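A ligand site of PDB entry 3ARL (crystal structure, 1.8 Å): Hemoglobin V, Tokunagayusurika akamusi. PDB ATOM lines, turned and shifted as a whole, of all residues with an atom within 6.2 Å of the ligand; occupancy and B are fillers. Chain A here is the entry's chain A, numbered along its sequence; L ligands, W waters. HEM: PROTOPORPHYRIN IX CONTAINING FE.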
ATOM      1  N   TYR A  35       9.573  18.075 -29.268  1.00  0.00           N
ATOM      2  CA  TYR A  35      10.343  18.449 -28.067  1.00  0.00           C
ATOM      3  C   TYR A  35      11.050  19.791 -28.201  1.00  0.00           C
ATOM      4  O   TYR A  35      10.947  20.647 -27.303  1.00  0.00           O
ATOM      5  CB  TYR A  35      11.354  17.316 -27.764  1.00  0.00           C
ATOM      6  CG  TYR A  35      12.418  17.647 -26.697  1.00  0.00           C
ATOM      7  CD1 TYR A  35      12.058  17.759 -25.360  1.00  0.00           C
ATOM      8  CD2 TYR A  35      13.785  17.755 -27.042  1.00  0.00           C
ATOM      9  CE1 TYR A  35      13.021  18.041 -24.382  1.00  0.00           C
ATOM     10  CE2 TYR A  35      14.741  18.025 -26.093  1.00  0.00           C
ATOM     11  CZ  TYR A  35      14.345  18.135 -24.764  1.00  0.00           C
ATOM     12  OH  TYR A  35      15.265  18.385 -23.782  1.00  0.00           O
ATOM     13  N   ASN A  42      16.374  24.101 -25.745  1.00  0.00           N
ATOM     14  CA  ASN A  42      17.208  22.900 -25.943  1.00  0.00           C
ATOM     15  C   ASN A  42      17.950  22.817 -27.282  1.00  0.00           C
ATOM     16  O   ASN A  42      18.937  22.091 -27.386  1.00  0.00           O
ATOM     17  CB  ASN A  42      16.366  21.647 -25.720  1.00  0.00           C
ATOM     18  CG  ASN A  42      15.955  21.528 -24.270  1.00  0.00           C
ATOM     19  OD1 ASN A  42      16.833  21.442 -23.397  1.00  0.00           O
ATOM     20  ND2 ASN A  42      14.654  21.658 -24.008  1.00  0.00           N
ATOM     21  N   LYS A  45      21.733  23.310 -27.347  1.00  0.00           N
ATOM     22  CA  LYS A  45      22.616  22.300 -26.739  1.00  0.00           C
ATOM     23  C   LYS A  45      23.219  21.392 -27.836  1.00  0.00           C
ATOM     24  O   LYS A  45      24.234  20.717 -27.611  1.00  0.00           O
ATOM     25  CB  LYS A  45      21.830  21.457 -25.696  1.00  0.00           C
ATOM     26  CG  LYS A  45      21.040  22.252 -24.693  1.00  0.00           C
ATOM     27  CD  LYS A  45      21.953  23.040 -23.710  1.00  0.00           C
ATOM     28  CE  LYS A  45      21.090  23.889 -22.715  1.00  0.00           C
ATOM     29  NZ  LYS A  45      21.982  24.453 -21.668  1.00  0.00           N
ATOM     30  N   PHE A  46      22.554  21.358 -29.003  1.00  0.00           N
ATOM     31  CA  PHE A  46      22.998  20.552 -30.158  1.00  0.00           C
ATOM     32  C   PHE A  46      23.807  21.435 -31.122  1.00  0.00           C
ATOM     33  O   PHE A  46      23.233  22.162 -31.926  1.00  0.00           O
ATOM     34  CB  PHE A  46      21.828  19.887 -30.869  1.00  0.00           C
ATOM     35  CG  PHE A  46      21.008  19.005 -29.955  1.00  0.00           C
ATOM     36  CD1 PHE A  46      21.312  17.660 -29.827  1.00  0.00           C
ATOM     37  CD2 PHE A  46      19.990  19.544 -29.171  1.00  0.00           C
ATOM     38  CE1 PHE A  46      20.567  16.841 -28.916  1.00  0.00           C
ATOM     39  CE2 PHE A  46      19.237  18.730 -28.275  1.00  0.00           C
ATOM     40  CZ  PHE A  46      19.529  17.385 -28.168  1.00  0.00           C
ATOM     41  N   GLU A  47      25.136  21.338 -31.042  1.00  0.00           N
ATOM     42  CA  GLU A  47      25.983  22.248 -31.827  1.00  0.00           C
ATOM     43  C   GLU A  47      25.764  22.186 -33.321  1.00  0.00           C
ATOM     44  O   GLU A  47      25.950  23.210 -34.017  1.00  0.00           O
ATOM     45  CB  GLU A  47      27.465  22.062 -31.505  1.00  0.00           C
ATOM     46  CG  GLU A  47      27.778  22.426 -30.063  1.00  0.00           C
ATOM     47  CD  GLU A  47      27.929  23.922 -29.848  1.00  0.00           C
ATOM     48  OE1 GLU A  47      27.905  24.714 -30.804  1.00  0.00           O
ATOM     49  OE2 GLU A  47      28.116  24.303 -28.686  1.00  0.00           O
ATOM     50  N   THR A  48      25.344  21.028 -33.825  1.00  0.00           N
ATOM     51  CA  THR A  48      25.044  20.913 -35.253  1.00  0.00           C
ATOM     52  C   THR A  48      23.747  21.622 -35.669  1.00  0.00           C
ATOM     53  O   THR A  48      23.550  21.924 -36.862  1.00  0.00           O
ATOM     54  CB  THR A  48      24.973  19.464 -35.762  1.00  0.00           C
ATOM     55  OG1 THR A  48      23.909  18.771 -35.097  1.00  0.00           O
ATOM     56  CG2 THR A  48      26.323  18.759 -35.578  1.00  0.00           C
ATOM     57  N   ILE A  66      20.388  12.869 -34.924  1.00  0.00           N
ATOM     58  CA  ILE A  66      20.218  13.100 -33.472  1.00  0.00           C
ATOM     59  C   ILE A  66      18.951  12.399 -32.977  1.00  0.00           C
ATOM     60  O   ILE A  66      19.000  11.665 -31.998  1.00  0.00           O
ATOM     61  CB  ILE A  66      20.171  14.621 -33.114  1.00  0.00           C
ATOM     62  CG1 ILE A  66      21.511  15.271 -33.481  1.00  0.00           C
ATOM     63  CG2 ILE A  66      19.764  14.831 -31.627  1.00  0.00           C
ATOM     64  CD1 ILE A  66      21.534  16.785 -33.545  1.00  0.00           C
ATOM     65  N   ARG A  69      19.423   8.635 -32.896  1.00  0.00           N
ATOM     66  CA  ARG A  69      20.339   8.102 -31.864  1.00  0.00           C
ATOM     67  C   ARG A  69      19.649   8.026 -30.492  1.00  0.00           C
ATOM     68  O   ARG A  69      19.877   7.083 -29.733  1.00  0.00           O
ATOM     69  CB  ARG A  69      21.653   8.890 -31.796  1.00  0.00           C
ATOM     70  CG  ARG A  69      21.551  10.183 -31.000  1.00  0.00           C
ATOM     71  CD  ARG A  69      22.698  11.110 -31.315  1.00  0.00           C
ATOM     72  NE  ARG A  69      22.658  12.331 -30.505  1.00  0.00           N
ATOM     73  CZ  ARG A  69      23.446  13.385 -30.750  1.00  0.00           C
ATOM     74  NH1 ARG A  69      24.293  13.305 -31.774  1.00  0.00           N
ATOM     75  NH2 ARG A  69      23.382  14.490 -30.000  1.00  0.00           N
ATOM     76  N   ILE A  70      18.769   9.002 -30.216  1.00  0.00           N
ATOM     77  CA  ILE A  70      18.022   9.001 -28.958  1.00  0.00           C
ATOM     78  C   ILE A  70      17.091   7.753 -28.927  1.00  0.00           C
ATOM     79  O   ILE A  70      17.068   6.941 -27.974  1.00  0.00           O
ATOM     80  CB  ILE A  70      17.171  10.289 -28.792  1.00  0.00           C
ATOM     81  CG1 ILE A  70      18.053  11.503 -28.514  1.00  0.00           C
ATOM     82  CG2 ILE A  70      16.141  10.134 -27.631  1.00  0.00           C
ATOM     83  CD1 ILE A  70      17.341  12.815 -28.761  1.00  0.00           C
ATOM     84  N   PHE A  71      16.315   7.618 -30.002  1.00  0.00           N
ATOM     85  CA  PHE A  71      15.348   6.516 -30.096  1.00  0.00           C
ATOM     86  C   PHE A  71      15.947   5.131 -30.186  1.00  0.00           C
ATOM     87  O   PHE A  71      15.378   4.169 -29.656  1.00  0.00           O
ATOM     88  CB  PHE A  71      14.333   6.831 -31.208  1.00  0.00           C
ATOM     89  CG  PHE A  71      13.186   7.629 -30.689  1.00  0.00           C
ATOM     90  CD1 PHE A  71      13.361   8.960 -30.287  1.00  0.00           C
ATOM     91  CD2 PHE A  71      11.935   7.023 -30.510  1.00  0.00           C
ATOM     92  CE1 PHE A  71      12.273   9.703 -29.755  1.00  0.00           C
ATOM     93  CE2 PHE A  71      10.863   7.755 -29.949  1.00  0.00           C
ATOM     94  CZ  PHE A  71      11.039   9.086 -29.561  1.00  0.00           C
ATOM     95  N   ILE A  73      18.723   4.249 -28.585  1.00  0.00           N
ATOM     96  CA  ILE A  73      18.989   3.911 -27.192  1.00  0.00           C
ATOM     97  C   ILE A  73      17.747   3.386 -26.507  1.00  0.00           C
ATOM     98  O   ILE A  73      17.804   2.337 -25.854  1.00  0.00           O
ATOM     99  CB  ILE A  73      19.627   5.085 -26.369  1.00  0.00           C
ATOM    100  CG1 ILE A  73      20.975   5.499 -26.962  1.00  0.00           C
ATOM    101  CG2 ILE A  73      19.743   4.718 -24.840  1.00  0.00           C
ATOM    102  CD1 ILE A  73      22.109   4.389 -26.845  1.00  0.00           C
ATOM    103  N   PHE A  74      16.629   4.125 -26.584  1.00  0.00           N
ATOM    104  CA  PHE A  74      15.405   3.591 -25.942  1.00  0.00           C
ATOM    105  C   PHE A  74      14.992   2.233 -26.550  1.00  0.00           C
ATOM    106  O   PHE A  74      14.564   1.333 -25.809  1.00  0.00           O
ATOM    107  CB  PHE A  74      14.272   4.607 -26.026  1.00  0.00           C
ATOM    108  CG  PHE A  74      14.475   5.787 -25.082  1.00  0.00           C
ATOM    109  CD1 PHE A  74      14.603   5.586 -23.689  1.00  0.00           C
ATOM    110  CD2 PHE A  74      14.525   7.087 -25.576  1.00  0.00           C
ATOM    111  CE1 PHE A  74      14.802   6.663 -22.812  1.00  0.00           C
ATOM    112  CE2 PHE A  74      14.727   8.130 -24.713  1.00  0.00           C
ATOM    113  CZ  PHE A  74      14.831   7.910 -23.308  1.00  0.00           C
ATOM    114  N   MET A  94      25.888   5.221 -23.156  1.00  0.00           N
ATOM    115  CA  MET A  94      25.463   6.495 -23.743  1.00  0.00           C
ATOM    116  C   MET A  94      25.650   7.667 -22.772  1.00  0.00           C
ATOM    117  O   MET A  94      25.667   8.802 -23.214  1.00  0.00           O
ATOM    118  CB  MET A  94      24.032   6.435 -24.304  1.00  0.00           C
ATOM    119  CG  MET A  94      22.965   6.028 -23.321  1.00  0.00           C
ATOM    120  SD  MET A  94      22.567   7.251 -22.054  1.00  0.00           S
ATOM    121  CE  MET A  94      22.119   8.592 -23.050  1.00  0.00           C
ATOM    122  N   PRO A  97      29.171  10.556 -23.026  1.00  0.00           N
ATOM    123  CA  PRO A  97      29.055  11.773 -23.825  1.00  0.00           C
ATOM    124  C   PRO A  97      28.278  12.924 -23.123  1.00  0.00           C
ATOM    125  O   PRO A  97      28.334  14.084 -23.550  1.00  0.00           O
ATOM    126  CB  PRO A  97      28.373  11.407 -25.143  1.00  0.00           C
ATOM    127  CG  PRO A  97      28.628   9.918 -25.367  1.00  0.00           C
ATOM    128  CD  PRO A  97      28.843   9.407 -23.867  1.00  0.00           C
ATOM    129  N   HIS A  98      27.330  12.555 -22.213  1.00  0.00           N
ATOM    130  CA  HIS A  98      26.516  13.589 -21.566  1.00  0.00           C
ATOM    131  C   HIS A  98      27.162  14.180 -20.299  1.00  0.00           C
ATOM    132  O   HIS A  98      26.705  15.180 -19.740  1.00  0.00           O
ATOM    133  CB  HIS A  98      25.163  12.973 -21.219  1.00  0.00           C
ATOM    134  CG  HIS A  98      24.444  12.569 -22.476  1.00  0.00           C
ATOM    135  ND1 HIS A  98      24.583  11.360 -23.057  1.00  0.00           N
ATOM    136  CD2 HIS A  98      23.516  13.314 -23.220  1.00  0.00           C
ATOM    137  CE1 HIS A  98      23.757  11.355 -24.115  1.00  0.00           C
ATOM    138  NE2 HIS A  98      23.104  12.517 -24.245  1.00  0.00           N
ATOM    139  N   ARG A 101      28.234  17.882 -19.805  1.00  0.00           N
ATOM    140  CA  ARG A 101      27.431  18.809 -20.604  1.00  0.00           C
ATOM    141  C   ARG A 101      26.472  19.615 -19.733  1.00  0.00           C
ATOM    142  O   ARG A 101      25.820  19.096 -18.833  1.00  0.00           O
ATOM    143  CB  ARG A 101      26.648  18.002 -21.633  1.00  0.00           C
ATOM    144  CG  ARG A 101      27.404  17.941 -22.942  1.00  0.00           C
ATOM    145  CD  ARG A 101      26.698  17.105 -24.012  1.00  0.00           C
ATOM    146  NE  ARG A 101      27.607  16.915 -25.130  1.00  0.00           N
ATOM    147  CZ  ARG A 101      28.181  18.016 -25.663  1.00  0.00           C
ATOM    148  NH1 ARG A 101      27.807  19.221 -25.252  1.00  0.00           N
ATOM    149  NH2 ARG A 101      29.127  17.888 -26.600  1.00  0.00           N
ATOM    150  N   ILE A 103      23.403  20.235 -19.433  1.00  0.00           N
ATOM    151  CA  ILE A 103      22.004  19.874 -19.676  1.00  0.00           C
ATOM    152  C   ILE A 103      21.342  19.557 -18.331  1.00  0.00           C
ATOM    153  O   ILE A 103      21.848  18.740 -17.546  1.00  0.00           O
ATOM    154  CB  ILE A 103      21.879  18.706 -20.667  1.00  0.00           C
ATOM    155  CG1 ILE A 103      22.632  19.056 -21.986  1.00  0.00           C
ATOM    156  CG2 ILE A 103      20.405  18.376 -20.939  1.00  0.00           C
ATOM    157  CD1 ILE A 103      22.852  17.913 -22.945  1.00  0.00           C
ATOM    158  N   SER A 107      15.546  19.323 -18.596  1.00  0.00           N
ATOM    159  CA  SER A 107      15.573  19.090 -20.059  1.00  0.00           C
ATOM    160  C   SER A 107      15.365  17.593 -20.396  1.00  0.00           C
ATOM    161  O   SER A 107      14.541  17.236 -21.259  1.00  0.00           O
ATOM    162  CB  SER A 107      16.901  19.584 -20.678  1.00  0.00           C
ATOM    163  OG  SER A 107      17.013  21.013 -20.650  1.00  0.00           O
ATOM    164  N   TYR A 108      16.131  16.719 -19.732  1.00  0.00           N
ATOM    165  CA  TYR A 108      15.924  15.283 -19.940  1.00  0.00           C
ATOM    166  C   TYR A 108      14.514  14.842 -19.555  1.00  0.00           C
ATOM    167  O   TYR A 108      13.880  14.036 -20.261  1.00  0.00           O
ATOM    168  CB  TYR A 108      16.893  14.475 -19.084  1.00  0.00           C
ATOM    169  CG  TYR A 108      18.357  14.738 -19.408  1.00  0.00           C
ATOM    170  CD1 TYR A 108      18.877  14.448 -20.681  1.00  0.00           C
ATOM    171  CD2 TYR A 108      19.216  15.192 -18.421  1.00  0.00           C
ATOM    172  CE1 TYR A 108      20.202  14.622 -20.990  1.00  0.00           C
ATOM    173  CE2 TYR A 108      20.605  15.393 -18.728  1.00  0.00           C
ATOM    174  CZ  TYR A 108      21.074  15.117 -19.988  1.00  0.00           C
ATOM    175  OH  TYR A 108      22.386  15.268 -20.356  1.00  0.00           O
ATOM    176  N   LEU A 111      11.959  15.699 -22.128  1.00  0.00           N
ATOM    177  CA  LEU A 111      11.968  14.744 -23.257  1.00  0.00           C
ATOM    178  C   LEU A 111      11.185  13.473 -22.898  1.00  0.00           C
ATOM    179  O   LEU A 111      10.370  12.999 -23.685  1.00  0.00           O
ATOM    180  CB  LEU A 111      13.409  14.419 -23.690  1.00  0.00           C
ATOM    181  CG  LEU A 111      13.591  13.346 -24.754  1.00  0.00           C
ATOM    182  CD1 LEU A 111      12.849  13.734 -26.082  1.00  0.00           C
ATOM    183  CD2 LEU A 111      15.084  13.128 -24.984  1.00  0.00           C
ATOM    184  N   ILE A 115       7.790  11.969 -24.930  1.00  0.00           N
ATOM    185  CA  ILE A 115       7.685  10.543 -25.304  1.00  0.00           C
ATOM    186  C   ILE A 115       6.418   9.920 -24.708  1.00  0.00           C
ATOM    187  O   ILE A 115       5.610   9.306 -25.428  1.00  0.00           O
ATOM    188  CB  ILE A 115       8.976   9.766 -24.954  1.00  0.00           C
ATOM    189  CG1 ILE A 115      10.177  10.316 -25.788  1.00  0.00           C
ATOM    190  CG2 ILE A 115       8.753   8.249 -25.172  1.00  0.00           C
ATOM    191  CD1 ILE A 115      11.591   9.759 -25.343  1.00  0.00           C
ATOM    192  N   PHE A 136      15.643   3.782 -16.071  1.00  0.00           N
ATOM    193  CA  PHE A 136      16.448   4.526 -17.032  1.00  0.00           C
ATOM    194  C   PHE A 136      17.092   5.763 -16.399  1.00  0.00           C
ATOM    195  O   PHE A 136      18.331   5.918 -16.421  1.00  0.00           O
ATOM    196  CB  PHE A 136      15.637   4.937 -18.276  1.00  0.00           C
ATOM    197  CG  PHE A 136      16.485   5.674 -19.321  1.00  0.00           C
ATOM    198  CD1 PHE A 136      16.728   7.051 -19.205  1.00  0.00           C
ATOM    199  CD2 PHE A 136      17.053   4.954 -20.399  1.00  0.00           C
ATOM    200  CE1 PHE A 136      17.507   7.752 -20.161  1.00  0.00           C
ATOM    201  CE2 PHE A 136      17.848   5.663 -21.382  1.00  0.00           C
ATOM    202  CZ  PHE A 136      18.078   7.038 -21.232  1.00  0.00           C
ATOM    203  N   PHE A 137      16.247   6.631 -15.863  1.00  0.00           N
ATOM    204  CA  PHE A 137      16.726   7.851 -15.178  1.00  0.00           C
ATOM    205  C   PHE A 137      17.595   7.645 -13.919  1.00  0.00           C
ATOM    206  O   PHE A 137      18.574   8.370 -13.750  1.00  0.00           O
ATOM    207  CB  PHE A 137      15.591   8.832 -15.002  1.00  0.00           C
ATOM    208  CG  PHE A 137      15.279   9.477 -16.303  1.00  0.00           C
ATOM    209  CD1 PHE A 137      16.132  10.478 -16.809  1.00  0.00           C
ATOM    210  CD2 PHE A 137      14.260   9.014 -17.110  1.00  0.00           C
ATOM    211  CE1 PHE A 137      15.926  11.030 -18.060  1.00  0.00           C
ATOM    212  CE2 PHE A 137      14.028   9.582 -18.361  1.00  0.00           C
ATOM    213  CZ  PHE A 137      14.868  10.581 -18.833  1.00  0.00           C
ATOM    214  N   PHE A 140      20.983   6.585 -15.482  1.00  0.00           N
ATOM    215  CA  PHE A 140      21.503   7.728 -16.199  1.00  0.00           C
ATOM    216  C   PHE A 140      22.016   8.798 -15.235  1.00  0.00           C
ATOM    217  O   PHE A 140      23.164   9.222 -15.331  1.00  0.00           O
ATOM    218  CB  PHE A 140      20.433   8.277 -17.129  1.00  0.00           C
ATOM    219  CG  PHE A 140      20.901   9.370 -18.055  1.00  0.00           C
ATOM    220  CD1 PHE A 140      22.012   9.187 -18.947  1.00  0.00           C
ATOM    221  CD2 PHE A 140      20.224  10.592 -18.085  1.00  0.00           C
ATOM    222  CE1 PHE A 140      22.404  10.216 -19.813  1.00  0.00           C
ATOM    223  CE2 PHE A 140      20.621  11.628 -18.986  1.00  0.00           C
ATOM    224  CZ  PHE A 140      21.698  11.447 -19.836  1.00  0.00           C
HETATM  225  CHA HEM L   1      24.771  12.645 -27.666  1.00  0.00           C
HETATM  226  CHB HEM L   1      21.250   9.508 -26.533  1.00  0.00           C
HETATM  227  CHC HEM L   1      18.957  13.030 -24.107  1.00  0.00           C
HETATM  228  CHD HEM L   1      22.046  16.291 -25.893  1.00  0.00           C
HETATM  229  C1A HEM L   1      24.015  11.488 -27.614  1.00  0.00           C
HETATM  230  C2A HEM L   1      24.316  10.197 -28.248  1.00  0.00           C
HETATM  231  C3A HEM L   1      23.334   9.326 -27.919  1.00  0.00           C
HETATM  232  C4A HEM L   1      22.386  10.035 -27.086  1.00  0.00           C
HETATM  233  CMA HEM L   1      23.206   7.843 -28.360  1.00  0.00           C
HETATM  234  CAA HEM L   1      25.514   9.888 -29.205  1.00  0.00           C
HETATM  235  CBA HEM L   1      26.881   9.977 -28.609  1.00  0.00           C
HETATM  236  CGA HEM L   1      27.614  11.142 -29.256  1.00  0.00           C
HETATM  237  O1A HEM L   1      27.939  11.147 -30.492  1.00  0.00           O
HETATM  238  O2A HEM L   1      27.895  12.083 -28.486  1.00  0.00           O
HETATM  239  C1B HEM L   1      20.355  10.169 -25.728  1.00  0.00           C
HETATM  240  C2B HEM L   1      19.226   9.563 -25.007  1.00  0.00           C
HETATM  241  C3B HEM L   1      18.608  10.533 -24.320  1.00  0.00           C
HETATM  242  C4B HEM L   1      19.311  11.790 -24.576  1.00  0.00           C
HETATM  243  CMB HEM L   1      18.833   8.059 -25.031  1.00  0.00           C
HETATM  244  CAB HEM L   1      17.382  10.419 -23.397  1.00  0.00           C
HETATM  245  CBB HEM L   1      17.328  11.057 -22.228  1.00  0.00           C
HETATM  246  C1C HEM L   1      19.512  14.235 -24.482  1.00  0.00           C
HETATM  247  C2C HEM L   1      18.959  15.585 -24.250  1.00  0.00           C
HETATM  248  C3C HEM L   1      19.826  16.494 -24.758  1.00  0.00           C
HETATM  249  C4C HEM L   1      20.943  15.741 -25.297  1.00  0.00           C
HETATM  250  CMC HEM L   1      17.597  15.833 -23.548  1.00  0.00           C
HETATM  251  CAC HEM L   1      19.776  18.060 -24.788  1.00  0.00           C
HETATM  252  CBC HEM L   1      18.866  18.752 -24.096  1.00  0.00           C
HETATM  253  C1D HEM L   1      23.101  15.627 -26.432  1.00  0.00           C
HETATM  254  C2D HEM L   1      24.308  16.232 -26.931  1.00  0.00           C
HETATM  255  C3D HEM L   1      25.184  15.111 -27.431  1.00  0.00           C
HETATM  256  C4D HEM L   1      24.406  13.903 -27.260  1.00  0.00           C
HETATM  257  CMD HEM L   1      24.480  17.777 -26.969  1.00  0.00           C
HETATM  258  CAD HEM L   1      26.699  15.171 -27.837  1.00  0.00           C
HETATM  259  CBD HEM L   1      26.799  14.960 -29.326  1.00  0.00           C
HETATM  260  CGD HEM L   1      26.299  16.247 -29.886  1.00  0.00           C
HETATM  261  O1D HEM L   1      27.047  17.261 -29.794  1.00  0.00           O
HETATM  262  O2D HEM L   1      25.140  16.248 -30.381  1.00  0.00           O
HETATM  263  NA  HEM L   1      22.832  11.342 -26.931  1.00  0.00           N
HETATM  264  NB  HEM L   1      20.344  11.520 -25.430  1.00  0.00           N
HETATM  265  NC  HEM L   1      20.714  14.392 -25.114  1.00  0.00           N
HETATM  266  ND  HEM L   1      23.182  14.256 -26.707  1.00  0.00           N
HETATM  267 FE   HEM L   1      21.803  12.870 -25.958  1.00  0.00          FE
HETATM  268  O   HOH W   1      22.145   5.317 -30.484  1.00  0.00           O
HETATM  269  O   HOH W   2      24.854  18.398 -32.326  1.00  0.00           O
HETATM  270  O   HOH W   3      26.299  19.631 -29.185  1.00  0.00           O
HETATM  271  O   HOH W   4      25.209  15.428 -33.253  1.00  0.00           O
HETATM  272  O   HOH W   5      28.002  18.622 -31.738  1.00  0.00           O
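A ring nitrogen (ND1) of His 98 is in hydrogen-bond range of the backbone carbonyl oxygen (O) of Met 94 (2.8 Å). The backbone carbonyl oxygen (O) of Pro 97 sits at hydrogen-bond distance from the guanidinium group (NE) of Arg 101. The side-chain amide nitrogen of Asn 42 lies close to the side-chain hydroxyl of Tyr 35 (3.3 Å). The side-chain hydroxyl (OG) of Ser 107 sits at hydrogen-bond distance from the side-chain amide oxygen (OD1) of Asn 42 (2.8 Å). The side-chain hydroxyl of Tyr 35 sits at hydrogen-bond distance from the backbone carbonyl oxygen of Ser 107.
OH of Tyr 35 touches CMC of the ligand, 3.5 Å away. Asn 42 touches the ligand (OD1 to CBC, 3.4 Å). O of Lys 45 touches CMD of the ligand, 3.0 Å away. Phe 46 touches the ligand (CE1 to CHD, 3.4 Å). O of Ile 70 touches CMB of the ligand, at 3.6 Å. Ile 73 touches the ligand. Phe 74 touches the ligand (CZ to CAB, 3.6 Å). CE of Met 94 touches C1B of the ligand, 3.6 Å away. CB of Pro 97 touches O2A of the ligand (3.4 Å). Ile 103 touches the ligand (CD1 to CHD, 3.5 Å). Tyr 108 touches the ligand (CD1 to CMC, 3.4 Å). Leu 111 touches the ligand (CD2 to CAB, 3.9 Å). Phe 136 touches the ligand (CE1 to CBB, 3.9 Å). Hydrophobic or aromatic side chains within 4 Å of the ligand: Phe 46, Ile 70, Ile 73, Phe 74, Met 94, Pro 97, His 98, Ile 103, Tyr 108, Leu 111 and Phe 136. Of the 24 residues printed, 16 come within 4 Å of the ligand.
An iron atom (FE) of the ligand is bound by a ring nitrogen (NE2) of His 98 (2.2 Å). O2D of the ligand is in salt-bridge range of NH2 of Arg 69, 2.5 Å away. The guanidinium group (NH2) of Arg 101 lies within salt-bridge range of an oxygen (O1D) of the ligand.
Water W3 lies within hydrogen-bond range of O1D of the ligand (2.6 Å), N of Glu 47 (2.8 Å) and O of Lys 45 (2.8 Å). Water W2 lies within hydrogen-bond range of O2D of the ligand, OG1 of Thr 48 and N of Glu 47. Water W4 bridges the guanidinium group (NH1) of Arg 69 (2.7 Å) and an oxygen (O2D) of the ligand (3.0 Å).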
